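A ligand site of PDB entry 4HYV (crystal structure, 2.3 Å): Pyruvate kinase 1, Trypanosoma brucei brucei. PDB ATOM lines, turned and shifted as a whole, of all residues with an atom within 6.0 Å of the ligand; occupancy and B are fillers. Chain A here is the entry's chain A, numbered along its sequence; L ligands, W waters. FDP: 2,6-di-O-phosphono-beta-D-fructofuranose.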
ATOM      1  N   VAL A 399       0.793  34.618 -21.266  1.00  0.00           N
ATOM      2  CA  VAL A 399       2.095  34.035 -21.035  1.00  0.00           C
ATOM      3  C   VAL A 399       2.083  32.556 -21.381  1.00  0.00           C
ATOM      4  O   VAL A 399       1.103  31.861 -21.115  1.00  0.00           O
ATOM      5  CB  VAL A 399       2.544  34.217 -19.576  1.00  0.00           C
ATOM      6  CG1 VAL A 399       1.598  33.494 -18.646  1.00  0.00           C
ATOM      7  CG2 VAL A 399       3.992  33.736 -19.409  1.00  0.00           C
ATOM      8  N   LEU A 400       3.143  32.091 -22.036  1.00  0.00           N
ATOM      9  CA  LEU A 400       3.404  30.649 -22.139  1.00  0.00           C
ATOM     10  C   LEU A 400       4.143  30.148 -20.920  1.00  0.00           C
ATOM     11  O   LEU A 400       5.244  30.595 -20.623  1.00  0.00           O
ATOM     12  CB  LEU A 400       4.245  30.347 -23.388  1.00  0.00           C
ATOM     13  CG  LEU A 400       3.458  30.262 -24.695  1.00  0.00           C
ATOM     14  CD1 LEU A 400       2.533  31.437 -24.860  1.00  0.00           C
ATOM     15  CD2 LEU A 400       4.425  30.156 -25.895  1.00  0.00           C
ATOM     16  N   SER A 401       3.568  29.155 -20.258  1.00  0.00           N
ATOM     17  CA  SER A 401       4.246  28.551 -19.105  1.00  0.00           C
ATOM     18  C   SER A 401       3.955  27.073 -19.051  1.00  0.00           C
ATOM     19  O   SER A 401       2.785  26.640 -19.013  1.00  0.00           O
ATOM     20  CB  SER A 401       3.816  29.218 -17.776  1.00  0.00           C
ATOM     21  OG  SER A 401       4.620  28.731 -16.684  1.00  0.00           O
ATOM     22  N   ASN A 402       5.001  26.282 -18.938  1.00  0.00           N
ATOM     23  CA  ASN A 402       4.813  24.842 -18.827  1.00  0.00           C
ATOM     24  C   ASN A 402       4.791  24.362 -17.390  1.00  0.00           C
ATOM     25  O   ASN A 402       3.980  23.482 -17.034  1.00  0.00           O
ATOM     26  CB  ASN A 402       5.859  24.109 -19.630  1.00  0.00           C
ATOM     27  CG  ASN A 402       5.902  24.582 -21.064  1.00  0.00           C
ATOM     28  OD1 ASN A 402       4.879  24.676 -21.687  1.00  0.00           O
ATOM     29  ND2 ASN A 402       7.054  25.048 -21.504  1.00  0.00           N
ATOM     30  N   THR A 403       5.676  24.921 -16.557  1.00  0.00           N
ATOM     31  CA  THR A 403       5.747  24.530 -15.139  1.00  0.00           C
ATOM     32  C   THR A 403       4.809  25.387 -14.321  1.00  0.00           C
ATOM     33  O   THR A 403       4.446  25.007 -13.214  1.00  0.00           O
ATOM     34  CB  THR A 403       7.150  24.703 -14.563  1.00  0.00           C
ATOM     35  OG1 THR A 403       7.551  26.091 -14.693  1.00  0.00           O
ATOM     36  CG2 THR A 403       8.164  23.781 -15.336  1.00  0.00           C
ATOM     37  N   GLY A 404       4.468  26.566 -14.835  1.00  0.00           N
ATOM     38  CA  GLY A 404       3.655  27.507 -14.069  1.00  0.00           C
ATOM     39  C   GLY A 404       4.505  28.617 -13.486  1.00  0.00           C
ATOM     40  O   GLY A 404       4.000  29.676 -13.161  1.00  0.00           O
ATOM     41  N   ARG A 405       5.817  28.438 -13.481  1.00  0.00           N
ATOM     42  CA  ARG A 405       6.732  29.449 -12.935  1.00  0.00           C
ATOM     43  C   ARG A 405       6.504  30.870 -13.500  1.00  0.00           C
ATOM     44  O   ARG A 405       6.488  31.859 -12.741  1.00  0.00           O
ATOM     45  CB  ARG A 405       8.177  29.007 -13.167  1.00  0.00           C
ATOM     46  CG  ARG A 405       9.221  29.756 -12.364  1.00  0.00           C
ATOM     47  CD  ARG A 405      10.494  28.905 -12.215  1.00  0.00           C
ATOM     48  NE  ARG A 405      10.221  27.521 -12.615  1.00  0.00           N
ATOM     49  CZ  ARG A 405      10.754  26.429 -12.061  1.00  0.00           C
ATOM     50  NH1 ARG A 405      10.378  25.235 -12.477  1.00  0.00           N
ATOM     51  NH2 ARG A 405      11.663  26.540 -11.102  1.00  0.00           N
ATOM     52  N   SER A 406       6.450  30.985 -14.825  1.00  0.00           N
ATOM     53  CA  SER A 406       6.351  32.295 -15.475  1.00  0.00           C
ATOM     54  C   SER A 406       4.973  32.932 -15.211  1.00  0.00           C
ATOM     55  O   SER A 406       4.875  34.158 -15.042  1.00  0.00           O
ATOM     56  CB  SER A 406       6.574  32.173 -16.991  1.00  0.00           C
ATOM     57  OG  SER A 406       7.872  31.612 -17.282  1.00  0.00           O
ATOM     58  N   ALA A 407       3.924  32.113 -15.129  1.00  0.00           N
ATOM     59  CA  ALA A 407       2.589  32.639 -14.756  1.00  0.00           C
ATOM     60  C   ALA A 407       2.585  33.180 -13.340  1.00  0.00           C
ATOM     61  O   ALA A 407       2.046  34.264 -13.085  1.00  0.00           O
ATOM     62  CB  ALA A 407       1.524  31.562 -14.913  1.00  0.00           C
ATOM     63  N   THR A 424       1.436  23.494 -21.380  1.00  0.00           N
ATOM     64  CA  THR A 424       1.482  22.193 -22.022  1.00  0.00           C
ATOM     65  C   THR A 424       1.186  21.057 -21.027  1.00  0.00           C
ATOM     66  O   THR A 424       1.240  19.889 -21.385  1.00  0.00           O
ATOM     67  CB  THR A 424       2.838  21.950 -22.730  1.00  0.00           C
ATOM     68  OG1 THR A 424       3.894  22.112 -21.787  1.00  0.00           O
ATOM     69  CG2 THR A 424       3.042  22.936 -23.838  1.00  0.00           C
ATOM     70  N   ARG A 425       0.829  21.417 -19.787  1.00  0.00           N
ATOM     71  CA  ARG A 425       0.585  20.444 -18.733  1.00  0.00           C
ATOM     72  C   ARG A 425      -0.716  20.699 -18.052  1.00  0.00           C
ATOM     73  O   ARG A 425      -0.918  21.754 -17.426  1.00  0.00           O
ATOM     74  CB  ARG A 425       1.713  20.447 -17.693  1.00  0.00           C
ATOM     75  CG  ARG A 425       3.026  19.937 -18.226  1.00  0.00           C
ATOM     76  CD  ARG A 425       4.091  19.890 -17.126  1.00  0.00           C
ATOM     77  NE  ARG A 425       5.401  20.214 -17.687  1.00  0.00           N
ATOM     78  CZ  ARG A 425       6.517  20.377 -16.983  1.00  0.00           C
ATOM     79  NH1 ARG A 425       6.498  20.245 -15.653  1.00  0.00           N
ATOM     80  NH2 ARG A 425       7.636  20.788 -17.605  1.00  0.00           N
ATOM     81  N   ASP A 451       5.515  23.352 -31.614  1.00  0.00           N
ATOM     82  CA  ASP A 451       5.318  24.809 -31.464  1.00  0.00           C
ATOM     83  C   ASP A 451       6.569  25.609 -31.044  1.00  0.00           C
ATOM     84  O   ASP A 451       6.474  26.542 -30.246  1.00  0.00           O
ATOM     85  CB  ASP A 451       4.135  25.117 -30.541  1.00  0.00           C
ATOM     86  CG  ASP A 451       3.528  26.516 -30.813  1.00  0.00           C
ATOM     87  OD1 ASP A 451       3.448  26.912 -31.997  1.00  0.00           O
ATOM     88  OD2 ASP A 451       3.120  27.195 -29.823  1.00  0.00           O
ATOM     89  N   LYS A 452       7.685  25.323 -31.691  1.00  0.00           N
ATOM     90  CA  LYS A 452       8.937  26.010 -31.420  1.00  0.00           C
ATOM     91  C   LYS A 452       8.833  27.522 -31.583  1.00  0.00           C
ATOM     92  O   LYS A 452       9.422  28.279 -30.827  1.00  0.00           O
ATOM     93  CB  LYS A 452      10.064  25.479 -32.314  1.00  0.00           C
ATOM     94  CG  LYS A 452      10.591  24.112 -31.885  1.00  0.00           C
ATOM     95  CD  LYS A 452      11.386  23.439 -33.007  1.00  0.00           C
ATOM     96  CE  LYS A 452      12.487  22.528 -32.472  1.00  0.00           C
ATOM     97  NZ  LYS A 452      11.992  21.677 -31.348  1.00  0.00           N
ATOM     98  N   LYS A 454       6.228  29.257 -31.221  1.00  0.00           N
ATOM     99  CA  LYS A 454       5.195  29.762 -30.286  1.00  0.00           C
ATOM    100  C   LYS A 454       3.870  30.128 -30.916  1.00  0.00           C
ATOM    101  O   LYS A 454       2.952  30.550 -30.226  1.00  0.00           O
ATOM    102  CB  LYS A 454       5.690  30.946 -29.423  1.00  0.00           C
ATOM    103  CG  LYS A 454       7.198  31.035 -29.184  1.00  0.00           C
ATOM    104  CD  LYS A 454       7.724  29.877 -28.372  1.00  0.00           C
ATOM    105  CE  LYS A 454       9.189  30.101 -28.002  1.00  0.00           C
ATOM    106  NZ  LYS A 454       9.906  28.788 -27.844  1.00  0.00           N
ATOM    107  N   ARG A 457       0.518  28.298 -29.743  1.00  0.00           N
ATOM    108  CA  ARG A 457       0.066  28.587 -28.395  1.00  0.00           C
ATOM    109  C   ARG A 457      -0.391  30.041 -28.259  1.00  0.00           C
ATOM    110  O   ARG A 457      -1.374  30.318 -27.569  1.00  0.00           O
ATOM    111  CB  ARG A 457       1.115  28.246 -27.363  1.00  0.00           C
ATOM    112  CG  ARG A 457       1.370  26.755 -27.278  1.00  0.00           C
ATOM    113  CD  ARG A 457       2.533  26.435 -26.395  1.00  0.00           C
ATOM    114  NE  ARG A 457       3.784  26.672 -27.090  1.00  0.00           N
ATOM    115  CZ  ARG A 457       4.973  26.633 -26.509  1.00  0.00           C
ATOM    116  NH1 ARG A 457       5.055  26.445 -25.181  1.00  0.00           N
ATOM    117  NH2 ARG A 457       6.090  26.731 -27.242  1.00  0.00           N
ATOM    118  N   VAL A 480       4.095  37.286 -23.369  1.00  0.00           N
ATOM    119  CA  VAL A 480       5.383  36.991 -22.753  1.00  0.00           C
ATOM    120  C   VAL A 480       5.728  35.531 -23.047  1.00  0.00           C
ATOM    121  O   VAL A 480       4.952  34.626 -22.748  1.00  0.00           O
ATOM    122  CB  VAL A 480       5.306  37.198 -21.216  1.00  0.00           C
ATOM    123  CG1 VAL A 480       6.575  36.723 -20.537  1.00  0.00           C
ATOM    124  CG2 VAL A 480       5.058  38.665 -20.891  1.00  0.00           C
ATOM    125  N   HIS A 481       6.838  35.319 -23.751  1.00  0.00           N
ATOM    126  CA  HIS A 481       7.403  33.971 -23.913  1.00  0.00           C
ATOM    127  C   HIS A 481       8.855  34.085 -24.347  1.00  0.00           C
ATOM    128  O   HIS A 481       9.467  35.135 -24.129  1.00  0.00           O
ATOM    129  CB  HIS A 481       6.566  33.142 -24.906  1.00  0.00           C
ATOM    130  CG  HIS A 481       6.334  33.825 -26.244  1.00  0.00           C
ATOM    131  ND1 HIS A 481       7.316  33.944 -27.194  1.00  0.00           N
ATOM    132  CD2 HIS A 481       5.159  34.335 -26.813  1.00  0.00           C
ATOM    133  CE1 HIS A 481       6.797  34.572 -28.287  1.00  0.00           C
ATOM    134  NE2 HIS A 481       5.470  34.779 -28.067  1.00  0.00           N
ATOM    135  N   ALA A 482       9.463  33.014 -24.840  1.00  0.00           N
ATOM    136  CA  ALA A 482      10.836  33.142 -25.353  1.00  0.00           C
ATOM    137  C   ALA A 482      10.853  33.521 -26.809  1.00  0.00           C
ATOM    138  O   ALA A 482       9.887  33.302 -27.526  1.00  0.00           O
ATOM    139  CB  ALA A 482      11.660  31.874 -25.115  1.00  0.00           C
ATOM    140  N   ASP A 483      11.913  34.176 -27.220  1.00  0.00           N
ATOM    141  CA  ASP A 483      12.195  34.292 -28.624  1.00  0.00           C
ATOM    142  C   ASP A 483      12.521  32.918 -29.241  1.00  0.00           C
ATOM    143  O   ASP A 483      12.461  31.890 -28.547  1.00  0.00           O
ATOM    144  CB  ASP A 483      13.312  35.307 -28.850  1.00  0.00           C
ATOM    145  CG  ASP A 483      14.691  34.797 -28.376  1.00  0.00           C
ATOM    146  OD1 ASP A 483      14.910  33.560 -28.273  1.00  0.00           O
ATOM    147  OD2 ASP A 483      15.596  35.650 -28.226  1.00  0.00           O
ATOM    148  N   VAL A 486      15.889  30.949 -27.102  1.00  0.00           N
ATOM    149  CA  VAL A 486      16.088  30.761 -25.676  1.00  0.00           C
ATOM    150  C   VAL A 486      15.186  29.675 -25.111  1.00  0.00           C
ATOM    151  O   VAL A 486      14.020  29.549 -25.527  1.00  0.00           O
ATOM    152  CB  VAL A 486      15.885  32.089 -24.935  1.00  0.00           C
ATOM    153  CG1 VAL A 486      15.779  31.853 -23.442  1.00  0.00           C
ATOM    154  CG2 VAL A 486      17.054  33.023 -25.265  1.00  0.00           C
ATOM    155  N   LYS A 487      15.766  28.775 -24.308  1.00  0.00           N
ATOM    156  CA  LYS A 487      14.987  27.713 -23.690  1.00  0.00           C
ATOM    157  C   LYS A 487      15.075  27.809 -22.184  1.00  0.00           C
ATOM    158  O   LYS A 487      16.157  27.953 -21.641  1.00  0.00           O
ATOM    159  CB  LYS A 487      15.473  26.336 -24.148  1.00  0.00           C
ATOM    160  CG  LYS A 487      15.586  26.172 -25.651  1.00  0.00           C
ATOM    161  CD  LYS A 487      14.273  25.698 -26.295  1.00  0.00           C
ATOM    162  CE  LYS A 487      14.348  25.807 -27.818  1.00  0.00           C
ATOM    163  NZ  LYS A 487      13.077  26.326 -28.424  1.00  0.00           N
ATOM    164  N   GLY A 488      13.951  27.585 -21.518  1.00  0.00           N
ATOM    165  CA  GLY A 488      13.963  27.429 -20.070  1.00  0.00           C
ATOM    166  C   GLY A 488      13.249  28.561 -19.369  1.00  0.00           C
ATOM    167  O   GLY A 488      12.776  28.411 -18.245  1.00  0.00           O
ATOM    168  N   TYR A 489      13.067  29.678 -20.067  1.00  0.00           N
ATOM    169  CA  TYR A 489      12.399  30.837 -19.427  1.00  0.00           C
ATOM    170  C   TYR A 489      11.946  31.802 -20.499  1.00  0.00           C
ATOM    171  O   TYR A 489      12.382  31.700 -21.657  1.00  0.00           O
ATOM    172  CB  TYR A 489      13.376  31.512 -18.454  1.00  0.00           C
ATOM    173  CG  TYR A 489      14.621  32.068 -19.106  1.00  0.00           C
ATOM    174  CD1 TYR A 489      15.748  31.254 -19.335  1.00  0.00           C
ATOM    175  CD2 TYR A 489      14.709  33.405 -19.436  1.00  0.00           C
ATOM    176  CE1 TYR A 489      16.887  31.773 -19.951  1.00  0.00           C
ATOM    177  CE2 TYR A 489      15.820  33.928 -20.048  1.00  0.00           C
ATOM    178  CZ  TYR A 489      16.918  33.118 -20.292  1.00  0.00           C
ATOM    179  OH  TYR A 489      18.025  33.669 -20.890  1.00  0.00           O
ATOM    180  N   PRO A 490      11.115  32.767 -20.125  1.00  0.00           N
ATOM    181  CA  PRO A 490      10.740  33.746 -21.152  1.00  0.00           C
ATOM    182  C   PRO A 490      11.750  34.891 -21.176  1.00  0.00           C
ATOM    183  O   PRO A 490      12.029  35.471 -20.147  1.00  0.00           O
ATOM    184  CB  PRO A 490       9.396  34.261 -20.651  1.00  0.00           C
ATOM    185  CG  PRO A 490       9.543  34.165 -19.148  1.00  0.00           C
ATOM    186  CD  PRO A 490      10.247  32.870 -18.930  1.00  0.00           C
HETATM  187  P1  FDP L   1       8.685  26.952 -24.628  1.00  0.00           P
HETATM  188  O1P FDP L   1       8.428  27.863 -25.760  1.00  0.00           O
HETATM  189  O2P FDP L   1       7.548  25.951 -24.336  1.00  0.00           O
HETATM  190  O3P FDP L   1      10.048  26.160 -24.891  1.00  0.00           O
HETATM  191  O1  FDP L   1      11.782  27.355 -23.168  1.00  0.00           O
HETATM  192  C1  FDP L   1      11.133  28.566 -23.649  1.00  0.00           C
HETATM  193  C2  FDP L   1       9.810  28.732 -22.886  1.00  0.00           C
HETATM  194  O2  FDP L   1       8.891  27.653 -23.139  1.00  0.00           O
HETATM  195  C3  FDP L   1       9.157  30.094 -23.151  1.00  0.00           C
HETATM  196  O3  FDP L   1       8.564  30.095 -24.465  1.00  0.00           O
HETATM  197  C4  FDP L   1       8.088  30.039 -22.082  1.00  0.00           C
HETATM  198  O4  FDP L   1       7.506  31.330 -21.830  1.00  0.00           O
HETATM  199  C5  FDP L   1       8.936  29.555 -20.860  1.00  0.00           C
HETATM  200  O5  FDP L   1      10.012  28.701 -21.460  1.00  0.00           O
HETATM  201  C6  FDP L   1       8.128  28.722 -19.924  1.00  0.00           C
HETATM  202  O6  FDP L   1       8.868  28.475 -18.743  1.00  0.00           O
HETATM  203  P2  FDP L   1       8.129  28.028 -17.417  1.00  0.00           P
HETATM  204  O4P FDP L   1       7.096  29.051 -16.908  1.00  0.00           O
HETATM  205  O5P FDP L   1       7.421  26.725 -17.814  1.00  0.00           O
HETATM  206  O6P FDP L   1       9.206  27.709 -16.276  1.00  0.00           O
HETATM  207  O   HOH W   1      11.197  23.932 -23.701  1.00  0.00           O
HETATM  208  O   HOH W   2      11.052  29.285 -16.258  1.00  0.00           O
HETATM  209  O   HOH W   3      11.438  26.075 -17.535  1.00  0.00           O
HETATM  210  O   HOH W   4      10.007  25.878 -27.760  1.00  0.00           O
HETATM  211  O   HOH W   5       7.238  23.363 -25.507  1.00  0.00           O
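The side-chain hydroxyl (OG) of Ser 401 lies within hydrogen-bond range of the backbone NH (N) of Arg 405.
The side-chain hydroxyl (OG) of Ser 401 is in hydrogen-bond range of the backbone NH (N) of Gly 404.
The backbone carbonyl oxygen (O) of Val 480 sits at hydrogen-bond distance from the backbone NH (N) of Leu 400 (3.2 Å).
The guanidinium group of Arg 457 is in salt-bridge range of the side-chain carboxylate of Asp 451 (2.9 Å).
The side-chain amide oxygen (OD1) of Asn 402 sits at hydrogen-bond distance from the side-chain hydroxyl (OG1) of Thr 424, at 2.7 Å.
The backbone carbonyl oxygen of Lys 452 lies within hydrogen-bond range of the side-chain amino group of Lys 454 (3.1 Å).
The backbone NH (N) of Arg 405 lies within hydrogen-bond range of the side-chain hydroxyl (OG1) of Thr 403, 3.2 Å away.
The backbone NH (N) of Val 486 lies within hydrogen-bond range of the side-chain carboxylate (OD1) of Asp 483 (3.0 Å).
The side-chain hydroxyl (OG) of Ser 401 is in hydrogen-bond range of an oxygen (O4P) of the ligand (2.5 Å).
O of Leu 400 is in hydrogen-bond range of O4 of the ligand.
An oxygen (O2P) of the ligand lies within salt-bridge range of the guanidinium group of Arg 457, 2.7 Å away.
N of Ser 406 sits at hydrogen-bond distance from O4P of the ligand, at 2.9 Å.
The side-chain hydroxyl (OG) of Ser 406 lies within hydrogen-bond range of an oxygen (O4P) of the ligand (2.7 Å).
The backbone NH (N) of Asn 402 lies within hydrogen-bond range of an oxygen (O5P) of the ligand, at 2.7 Å.
An oxygen (O2P) of the ligand lies within hydrogen-bond range of the side-chain amide nitrogen (ND2) of Asn 402.
The side-chain amino group of Lys 454 lies within salt-bridge range of an oxygen (O1P) of the ligand (2.7 Å).
O1 of the ligand is in hydrogen-bond range of N of Gly 488.
The backbone NH (N) of Thr 403 sits at hydrogen-bond distance from an oxygen (O5P) of the ligand (2.8 Å).
OG1 of Thr 403 is in hydrogen-bond range of O6P of the ligand, 2.8 Å away.
O3 of the ligand sits at hydrogen-bond distance from N of Ala 482, 3.1 Å away.
N of Tyr 489 sits at hydrogen-bond distance from O5 of the ligand (3.5 Å).
The guanidinium group (NE) of Arg 405 lies within salt-bridge range of an oxygen (O6P) of the ligand.
Water W2 bridges O6P of the ligand and O of Gly 488.
Water W4 lies within hydrogen-bond range of O3P of the ligand (2.9 Å), NZ of Lys 454 (2.9 Å) and NZ of Lys 487 (3.2 Å).
Water W3 lies within hydrogen-bond range of the backbone carbonyl oxygen (O) of Gly 488 (2.8 Å) and an oxygen (O6P) of the ligand (3.0 Å).
Residues that only touch the ligand: His 481, Val 486, Lys 487 and Pro 490.
Hydrophobic or aromatic side chains within 4 Å of the ligand: Leu 400, His 481, Ala 482 and Pro 490.
Of the 24 residues printed, 15 come within 4 Å of the ligand.
The nearest printed residue that does not touch the ligand is Gly 404 (4.2 Å).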
